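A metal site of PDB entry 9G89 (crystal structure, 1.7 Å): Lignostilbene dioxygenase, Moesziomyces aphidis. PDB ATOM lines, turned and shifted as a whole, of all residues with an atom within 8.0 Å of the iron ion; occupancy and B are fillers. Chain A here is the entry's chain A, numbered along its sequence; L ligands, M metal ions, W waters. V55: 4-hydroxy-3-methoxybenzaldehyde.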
ATOM      1  N   LEU A  49       9.037 -14.662 -20.182  1.00  0.00           N
ATOM      2  CA  LEU A  49       9.768 -14.886 -18.929  1.00  0.00           C
ATOM      3  C   LEU A  49      11.259 -15.172 -19.152  1.00  0.00           C
ATOM      4  O   LEU A  49      12.098 -14.946 -18.274  1.00  0.00           O
ATOM      5  CB  LEU A  49       9.120 -16.025 -18.152  1.00  0.00           C
ATOM      6  CG  LEU A  49       7.899 -15.676 -17.292  1.00  0.00           C
ATOM      7  CD1 LEU A  49       7.521 -17.061 -16.765  1.00  0.00           C
ATOM      8  CD2 LEU A  49       8.245 -14.718 -16.153  1.00  0.00           C
ATOM      9  N   THR A 164      -1.197 -19.080 -19.103  1.00  0.00           N
ATOM     10  CA  THR A 164      -0.299 -19.648 -18.094  1.00  0.00           C
ATOM     11  C   THR A 164      -0.248 -21.169 -18.219  1.00  0.00           C
ATOM     12  O   THR A 164       0.836 -21.732 -18.205  1.00  0.00           O
ATOM     13  CB  THR A 164      -0.791 -19.263 -16.677  1.00  0.00           C
ATOM     14  OG1 THR A 164      -0.688 -17.830 -16.660  1.00  0.00           O
ATOM     15  CG2 THR A 164       0.031 -19.901 -15.583  1.00  0.00           C
ATOM     16  N   ASN A 165      -1.392 -21.847 -18.331  1.00  0.00           N
ATOM     17  CA  ASN A 165      -1.348 -23.307 -18.306  1.00  0.00           C
ATOM     18  C   ASN A 165      -2.578 -23.868 -19.000  1.00  0.00           C
ATOM     19  O   ASN A 165      -3.535 -23.143 -19.285  1.00  0.00           O
ATOM     20  CB  ASN A 165      -1.278 -23.777 -16.855  1.00  0.00           C
ATOM     21  CG  ASN A 165      -0.853 -25.221 -16.668  1.00  0.00           C
ATOM     22  OD1 ASN A 165      -0.444 -25.924 -17.604  1.00  0.00           O
ATOM     23  ND2 ASN A 165      -0.926 -25.676 -15.433  1.00  0.00           N
ATOM     24  N   GLU A 178      -4.828 -17.101 -13.679  1.00  0.00           N
ATOM     25  CA  GLU A 178      -5.425 -17.084 -12.353  1.00  0.00           C
ATOM     26  C   GLU A 178      -6.306 -15.876 -12.091  1.00  0.00           C
ATOM     27  O   GLU A 178      -6.933 -15.849 -11.012  1.00  0.00           O
ATOM     28  CB  GLU A 178      -4.315 -17.197 -11.310  1.00  0.00           C
ATOM     29  CG  GLU A 178      -3.395 -15.969 -11.211  1.00  0.00           C
ATOM     30  CD  GLU A 178      -2.078 -16.498 -10.641  1.00  0.00           C
ATOM     31  OE1 GLU A 178      -1.329 -17.231 -11.321  1.00  0.00           O
ATOM     32  OE2 GLU A 178      -1.785 -16.178  -9.473  1.00  0.00           O
ATOM     33  N   THR A 206      -7.522 -20.814 -10.384  1.00  0.00           N
ATOM     34  CA  THR A 206      -6.083 -21.045 -10.489  1.00  0.00           C
ATOM     35  C   THR A 206      -5.733 -21.607 -11.878  1.00  0.00           C
ATOM     36  O   THR A 206      -6.534 -22.366 -12.510  1.00  0.00           O
ATOM     37  CB  THR A 206      -5.683 -22.007  -9.365  1.00  0.00           C
ATOM     38  OG1 THR A 206      -4.255 -22.083  -9.411  1.00  0.00           O
ATOM     39  CG2 THR A 206      -6.195 -23.421  -9.553  1.00  0.00           C
ATOM     40  N   ALA A 207      -4.512 -21.304 -12.322  1.00  0.00           N
ATOM     41  CA  ALA A 207      -3.950 -21.960 -13.513  1.00  0.00           C
ATOM     42  C   ALA A 207      -3.213 -23.217 -13.102  1.00  0.00           C
ATOM     43  O   ALA A 207      -2.625 -23.850 -13.975  1.00  0.00           O
ATOM     44  CB  ALA A 207      -3.035 -21.018 -14.267  1.00  0.00           C
ATOM     45  N   HIS A 208      -3.266 -23.574 -11.792  1.00  0.00           N
ATOM     46  CA  HIS A 208      -2.624 -24.782 -11.296  1.00  0.00           C
ATOM     47  C   HIS A 208      -3.609 -25.725 -10.610  1.00  0.00           C
ATOM     48  O   HIS A 208      -3.324 -26.207  -9.522  1.00  0.00           O
ATOM     49  CB  HIS A 208      -1.423 -24.411 -10.409  1.00  0.00           C
ATOM     50  CG  HIS A 208      -0.245 -23.972 -11.229  1.00  0.00           C
ATOM     51  ND1 HIS A 208       0.437 -24.889 -12.008  1.00  0.00           N
ATOM     52  CD2 HIS A 208       0.301 -22.757 -11.465  1.00  0.00           C
ATOM     53  CE1 HIS A 208       1.409 -24.260 -12.655  1.00  0.00           C
ATOM     54  NE2 HIS A 208       1.362 -22.947 -12.315  1.00  0.00           N
ATOM     55  N   LYS A 210      -5.217 -29.444  -9.943  1.00  0.00           N
ATOM     56  CA  LYS A 210      -4.502 -30.707  -9.930  1.00  0.00           C
ATOM     57  C   LYS A 210      -5.523 -31.818 -10.179  1.00  0.00           C
ATOM     58  O   LYS A 210      -6.599 -31.817  -9.554  1.00  0.00           O
ATOM     59  CB  LYS A 210      -3.899 -30.893  -8.533  1.00  0.00           C
ATOM     60  CG  LYS A 210      -2.962 -29.768  -8.028  1.00  0.00           C
ATOM     61  CD  LYS A 210      -1.729 -29.465  -8.891  1.00  0.00           C
ATOM     62  CE  LYS A 210      -1.059 -28.195  -8.401  1.00  0.00           C
ATOM     63  NZ  LYS A 210       0.141 -27.852  -9.214  1.00  0.00           N
ATOM     64  N   HIS A 259      -0.258 -18.502  -6.442  1.00  0.00           N
ATOM     65  CA  HIS A 259      -0.095 -18.969  -7.811  1.00  0.00           C
ATOM     66  C   HIS A 259      -0.335 -20.480  -7.925  1.00  0.00           C
ATOM     67  O   HIS A 259      -0.976 -20.918  -8.875  1.00  0.00           O
ATOM     68  CB  HIS A 259       1.338 -18.670  -8.299  1.00  0.00           C
ATOM     69  CG  HIS A 259       1.545 -19.108  -9.709  1.00  0.00           C
ATOM     70  ND1 HIS A 259       0.866 -18.527 -10.761  1.00  0.00           N
ATOM     71  CD2 HIS A 259       2.343 -20.053 -10.272  1.00  0.00           C
ATOM     72  CE1 HIS A 259       1.228 -19.118 -11.892  1.00  0.00           C
ATOM     73  NE2 HIS A 259       2.140 -20.010 -11.636  1.00  0.00           N
ATOM     74  N   ASP A 260       0.223 -21.242  -6.971  1.00  0.00           N
ATOM     75  CA  ASP A 260       0.235 -22.693  -7.099  1.00  0.00           C
ATOM     76  C   ASP A 260      -0.242 -23.311  -5.768  1.00  0.00           C
ATOM     77  O   ASP A 260      -0.430 -22.629  -4.758  1.00  0.00           O
ATOM     78  CB  ASP A 260       1.619 -23.132  -7.555  1.00  0.00           C
ATOM     79  CG  ASP A 260       1.760 -24.524  -8.170  1.00  0.00           C
ATOM     80  OD1 ASP A 260       0.738 -25.253  -8.288  1.00  0.00           O
ATOM     81  OD2 ASP A 260       2.893 -24.868  -8.607  1.00  0.00           O
ATOM     82  N   TRP A 273       2.649 -16.546  -2.027  1.00  0.00           N
ATOM     83  CA  TRP A 273       3.825 -15.726  -2.259  1.00  0.00           C
ATOM     84  C   TRP A 273       3.730 -14.440  -1.457  1.00  0.00           C
ATOM     85  O   TRP A 273       2.632 -13.941  -1.203  1.00  0.00           O
ATOM     86  CB  TRP A 273       3.932 -15.348  -3.738  1.00  0.00           C
ATOM     87  CG  TRP A 273       4.203 -16.526  -4.646  1.00  0.00           C
ATOM     88  CD1 TRP A 273       4.471 -17.818  -4.361  1.00  0.00           C
ATOM     89  CD2 TRP A 273       4.250 -16.406  -6.077  1.00  0.00           C
ATOM     90  NE1 TRP A 273       4.641 -18.545  -5.520  1.00  0.00           N
ATOM     91  CE2 TRP A 273       4.532 -17.691  -6.595  1.00  0.00           C
ATOM     92  CE3 TRP A 273       4.062 -15.331  -6.964  1.00  0.00           C
ATOM     93  CZ2 TRP A 273       4.636 -17.931  -7.961  1.00  0.00           C
ATOM     94  CZ3 TRP A 273       4.190 -15.557  -8.317  1.00  0.00           C
ATOM     95  CH2 TRP A 273       4.469 -16.848  -8.814  1.00  0.00           C
ATOM     96  N   ILE A 323       8.059 -20.855  -6.140  1.00  0.00           N
ATOM     97  CA  ILE A 323       7.269 -20.442  -7.302  1.00  0.00           C
ATOM     98  C   ILE A 323       6.274 -21.534  -7.683  1.00  0.00           C
ATOM     99  O   ILE A 323       5.102 -21.224  -7.858  1.00  0.00           O
ATOM    100  CB  ILE A 323       8.180 -20.013  -8.468  1.00  0.00           C
ATOM    101  CG1 ILE A 323       9.105 -18.891  -8.046  1.00  0.00           C
ATOM    102  CG2 ILE A 323       7.357 -19.630  -9.725  1.00  0.00           C
ATOM    103  CD1 ILE A 323      10.265 -18.724  -9.032  1.00  0.00           C
ATOM    104  N   HIS A 324       6.746 -22.778  -7.786  1.00  0.00           N
ATOM    105  CA  HIS A 324       5.945 -23.902  -8.237  1.00  0.00           C
ATOM    106  C   HIS A 324       6.204 -25.115  -7.367  1.00  0.00           C
ATOM    107  O   HIS A 324       7.346 -25.366  -6.990  1.00  0.00           O
ATOM    108  CB  HIS A 324       6.307 -24.298  -9.677  1.00  0.00           C
ATOM    109  CG  HIS A 324       5.734 -23.323 -10.668  1.00  0.00           C
ATOM    110  ND1 HIS A 324       6.561 -22.589 -11.490  1.00  0.00           N
ATOM    111  CD2 HIS A 324       4.484 -22.991 -10.985  1.00  0.00           C
ATOM    112  CE1 HIS A 324       5.822 -21.830 -12.298  1.00  0.00           C
ATOM    113  NE2 HIS A 324       4.563 -22.035 -11.981  1.00  0.00           N
ATOM    114  N   THR A 325       5.148 -25.878  -7.166  1.00  0.00           N
ATOM    115  CA  THR A 325       5.290 -27.166  -6.525  1.00  0.00           C
ATOM    116  C   THR A 325       5.567 -28.231  -7.587  1.00  0.00           C
ATOM    117  O   THR A 325       5.103 -28.117  -8.724  1.00  0.00           O
ATOM    118  CB  THR A 325       4.079 -27.501  -5.679  1.00  0.00           C
ATOM    119  OG1 THR A 325       2.967 -27.647  -6.564  1.00  0.00           O
ATOM    120  CG2 THR A 325       3.818 -26.508  -4.561  1.00  0.00           C
ATOM    121  N   PHE A 348      10.179 -11.954  -9.398  1.00  0.00           N
ATOM    122  CA  PHE A 348       9.480 -11.038 -10.279  1.00  0.00           C
ATOM    123  C   PHE A 348       9.848  -9.608  -9.901  1.00  0.00           C
ATOM    124  O   PHE A 348       9.011  -8.849  -9.373  1.00  0.00           O
ATOM    125  CB  PHE A 348       7.940 -11.172 -10.155  1.00  0.00           C
ATOM    126  CG  PHE A 348       7.255 -12.377 -10.787  1.00  0.00           C
ATOM    127  CD1 PHE A 348       7.962 -13.297 -11.582  1.00  0.00           C
ATOM    128  CD2 PHE A 348       5.876 -12.521 -10.617  1.00  0.00           C
ATOM    129  CE1 PHE A 348       7.278 -14.321 -12.240  1.00  0.00           C
ATOM    130  CE2 PHE A 348       5.196 -13.579 -11.251  1.00  0.00           C
ATOM    131  CZ  PHE A 348       5.903 -14.468 -12.033  1.00  0.00           C
ATOM    132  N   GLU A 399      13.189 -24.606 -11.675  1.00  0.00           N
ATOM    133  CA  GLU A 399      11.854 -24.075 -11.893  1.00  0.00           C
ATOM    134  C   GLU A 399      11.083 -25.077 -12.746  1.00  0.00           C
ATOM    135  O   GLU A 399      11.621 -26.102 -13.150  1.00  0.00           O
ATOM    136  CB  GLU A 399      11.855 -22.601 -12.351  1.00  0.00           C
ATOM    137  CG  GLU A 399      11.193 -21.666 -11.312  1.00  0.00           C
ATOM    138  CD  GLU A 399       9.763 -22.116 -11.082  1.00  0.00           C
ATOM    139  OE1 GLU A 399       9.027 -22.107 -12.071  1.00  0.00           O
ATOM    140  OE2 GLU A 399       9.398 -22.640 -10.017  1.00  0.00           O
ATOM    141  N   PHE A 400       9.794 -24.769 -12.963  1.00  0.00           N
ATOM    142  CA  PHE A 400       8.868 -25.509 -13.807  1.00  0.00           C
ATOM    143  C   PHE A 400       8.992 -27.015 -13.581  1.00  0.00           C
ATOM    144  O   PHE A 400       9.234 -27.759 -14.526  1.00  0.00           O
ATOM    145  CB  PHE A 400       9.121 -25.198 -15.294  1.00  0.00           C
ATOM    146  CG  PHE A 400       8.783 -23.735 -15.600  1.00  0.00           C
ATOM    147  CD1 PHE A 400       7.456 -23.297 -15.523  1.00  0.00           C
ATOM    148  CD2 PHE A 400       9.788 -22.845 -15.997  1.00  0.00           C
ATOM    149  CE1 PHE A 400       7.131 -21.969 -15.830  1.00  0.00           C
ATOM    150  CE2 PHE A 400       9.477 -21.522 -16.308  1.00  0.00           C
ATOM    151  CZ  PHE A 400       8.143 -21.087 -16.247  1.00  0.00           C
ATOM    152  N   PHE A 432      14.142 -17.373 -14.297  1.00  0.00           N
ATOM    153  CA  PHE A 432      13.395 -17.784 -15.505  1.00  0.00           C
ATOM    154  C   PHE A 432      14.247 -17.647 -16.774  1.00  0.00           C
ATOM    155  O   PHE A 432      13.784 -18.039 -17.857  1.00  0.00           O
ATOM    156  CB  PHE A 432      12.135 -16.916 -15.646  1.00  0.00           C
ATOM    157  CG  PHE A 432      11.144 -17.199 -14.523  1.00  0.00           C
ATOM    158  CD1 PHE A 432      10.422 -18.406 -14.496  1.00  0.00           C
ATOM    159  CD2 PHE A 432      10.947 -16.236 -13.514  1.00  0.00           C
ATOM    160  CE1 PHE A 432       9.529 -18.672 -13.452  1.00  0.00           C
ATOM    161  CE2 PHE A 432      10.057 -16.488 -12.498  1.00  0.00           C
ATOM    162  CZ  PHE A 432       9.345 -17.693 -12.469  1.00  0.00           C
ATOM    163  N   GLU A 461       9.932 -25.976 -19.796  1.00  0.00           N
ATOM    164  CA  GLU A 461       9.404 -26.970 -18.833  1.00  0.00           C
ATOM    165  C   GLU A 461       9.271 -28.348 -19.462  1.00  0.00           C
ATOM    166  O   GLU A 461       8.739 -28.488 -20.574  1.00  0.00           O
ATOM    167  CB  GLU A 461       8.027 -26.477 -18.370  1.00  0.00           C
ATOM    168  CG  GLU A 461       7.332 -27.478 -17.453  1.00  0.00           C
ATOM    169  CD  GLU A 461       5.881 -27.069 -17.267  1.00  0.00           C
ATOM    170  OE1 GLU A 461       5.219 -26.922 -18.321  1.00  0.00           O
ATOM    171  OE2 GLU A 461       5.441 -26.923 -16.081  1.00  0.00           O
ATOM    172  N   ILE A 517       5.210 -20.730 -20.750  1.00  0.00           N
ATOM    173  CA  ILE A 517       5.050 -20.863 -19.317  1.00  0.00           C
ATOM    174  C   ILE A 517       4.912 -22.364 -19.059  1.00  0.00           C
ATOM    175  O   ILE A 517       5.933 -23.038 -18.970  1.00  0.00           O
ATOM    176  CB  ILE A 517       3.874 -19.998 -18.814  1.00  0.00           C
ATOM    177  CG1 ILE A 517       3.861 -18.599 -19.448  1.00  0.00           C
ATOM    178  CG2 ILE A 517       3.828 -19.965 -17.284  1.00  0.00           C
ATOM    179  CD1 ILE A 517       4.952 -17.649 -19.048  1.00  0.00           C
ATOM    180  N   HIS A 518       3.671 -22.905 -18.993  1.00  0.00           N
ATOM    181  CA  HIS A 518       3.530 -24.342 -18.838  1.00  0.00           C
ATOM    182  C   HIS A 518       3.115 -25.022 -20.129  1.00  0.00           C
ATOM    183  O   HIS A 518       2.664 -24.397 -21.113  1.00  0.00           O
ATOM    184  CB  HIS A 518       2.507 -24.619 -17.723  1.00  0.00           C
ATOM    185  CG  HIS A 518       2.937 -24.014 -16.419  1.00  0.00           C
ATOM    186  ND1 HIS A 518       3.913 -24.625 -15.653  1.00  0.00           N
ATOM    187  CD2 HIS A 518       2.564 -22.878 -15.753  1.00  0.00           C
ATOM    188  CE1 HIS A 518       4.125 -23.891 -14.556  1.00  0.00           C
ATOM    189  NE2 HIS A 518       3.343 -22.822 -14.610  1.00  0.00           N
HETATM  190  CAI V55 L   1       3.005 -16.689 -13.176  1.00  0.00           C
HETATM  191  CAG V55 L   1       2.621 -16.609 -14.534  1.00  0.00           C
HETATM  192  CAK V55 L   1       1.537 -15.834 -14.922  1.00  0.00           C
HETATM  193  CAJ V55 L   1       0.740 -15.222 -13.946  1.00  0.00           C
HETATM  194  CAF V55 L   1       1.092 -15.333 -12.602  1.00  0.00           C
HETATM  195  OAB V55 L   1       4.772 -18.190 -13.651  1.00  0.00           O
HETATM  196  CAE V55 L   1       2.239 -16.049 -12.229  1.00  0.00           C
HETATM  197  CAD V55 L   1       4.193 -17.470 -12.821  1.00  0.00           C
HETATM  198  CAA V55 L   1       1.927 -16.233 -17.256  1.00  0.00           C
HETATM  199  OAH V55 L   1       1.105 -15.695 -16.226  1.00  0.00           O
HETATM  200  OAC V55 L   1      -0.390 -14.543 -14.300  1.00  0.00           O
HETATM  201 FE    FE M   1       2.778 -21.493 -13.011  1.00  0.00          FE
HETATM  202  O   HOH W   1       3.283 -19.978 -14.230  1.00  0.00           O
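The nearest printed residue that does not touch the iron ion is Thr 164 (4.1 Å).
The iron ion is bound by water W1 (2.0 Å), NE2 of His 259 (2.1 Å), NE2 of His 324 (2.1 Å), NE2 of His 208 (2.1 Å) and NE2 of His 518 (2.2 Å). The iron ion has five donor atoms within binding distance.
OG1 of Thr 164 is in hydrogen-bond range of OAH of the ligand (2.8 Å).
ND1 of His 259 lies within hydrogen-bond range of OE1 of Glu 178 (2.6 Å). The side-chain carboxylate of Glu 399 sits at hydrogen-bond distance from a ring nitrogen (ND1) of His 324, 2.6 Å away. The backbone NH (N) of His 208 is in hydrogen-bond range of the side-chain hydroxyl (OG1) of Thr 206, at 3.0 Å. The backbone NH (N) of His 518 is in hydrogen-bond range of the backbone carbonyl oxygen (O) of Thr 164, at 3.2 Å. ND1 of His 518 lies within hydrogen-bond range of OE2 of Glu 461 (2.8 Å).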
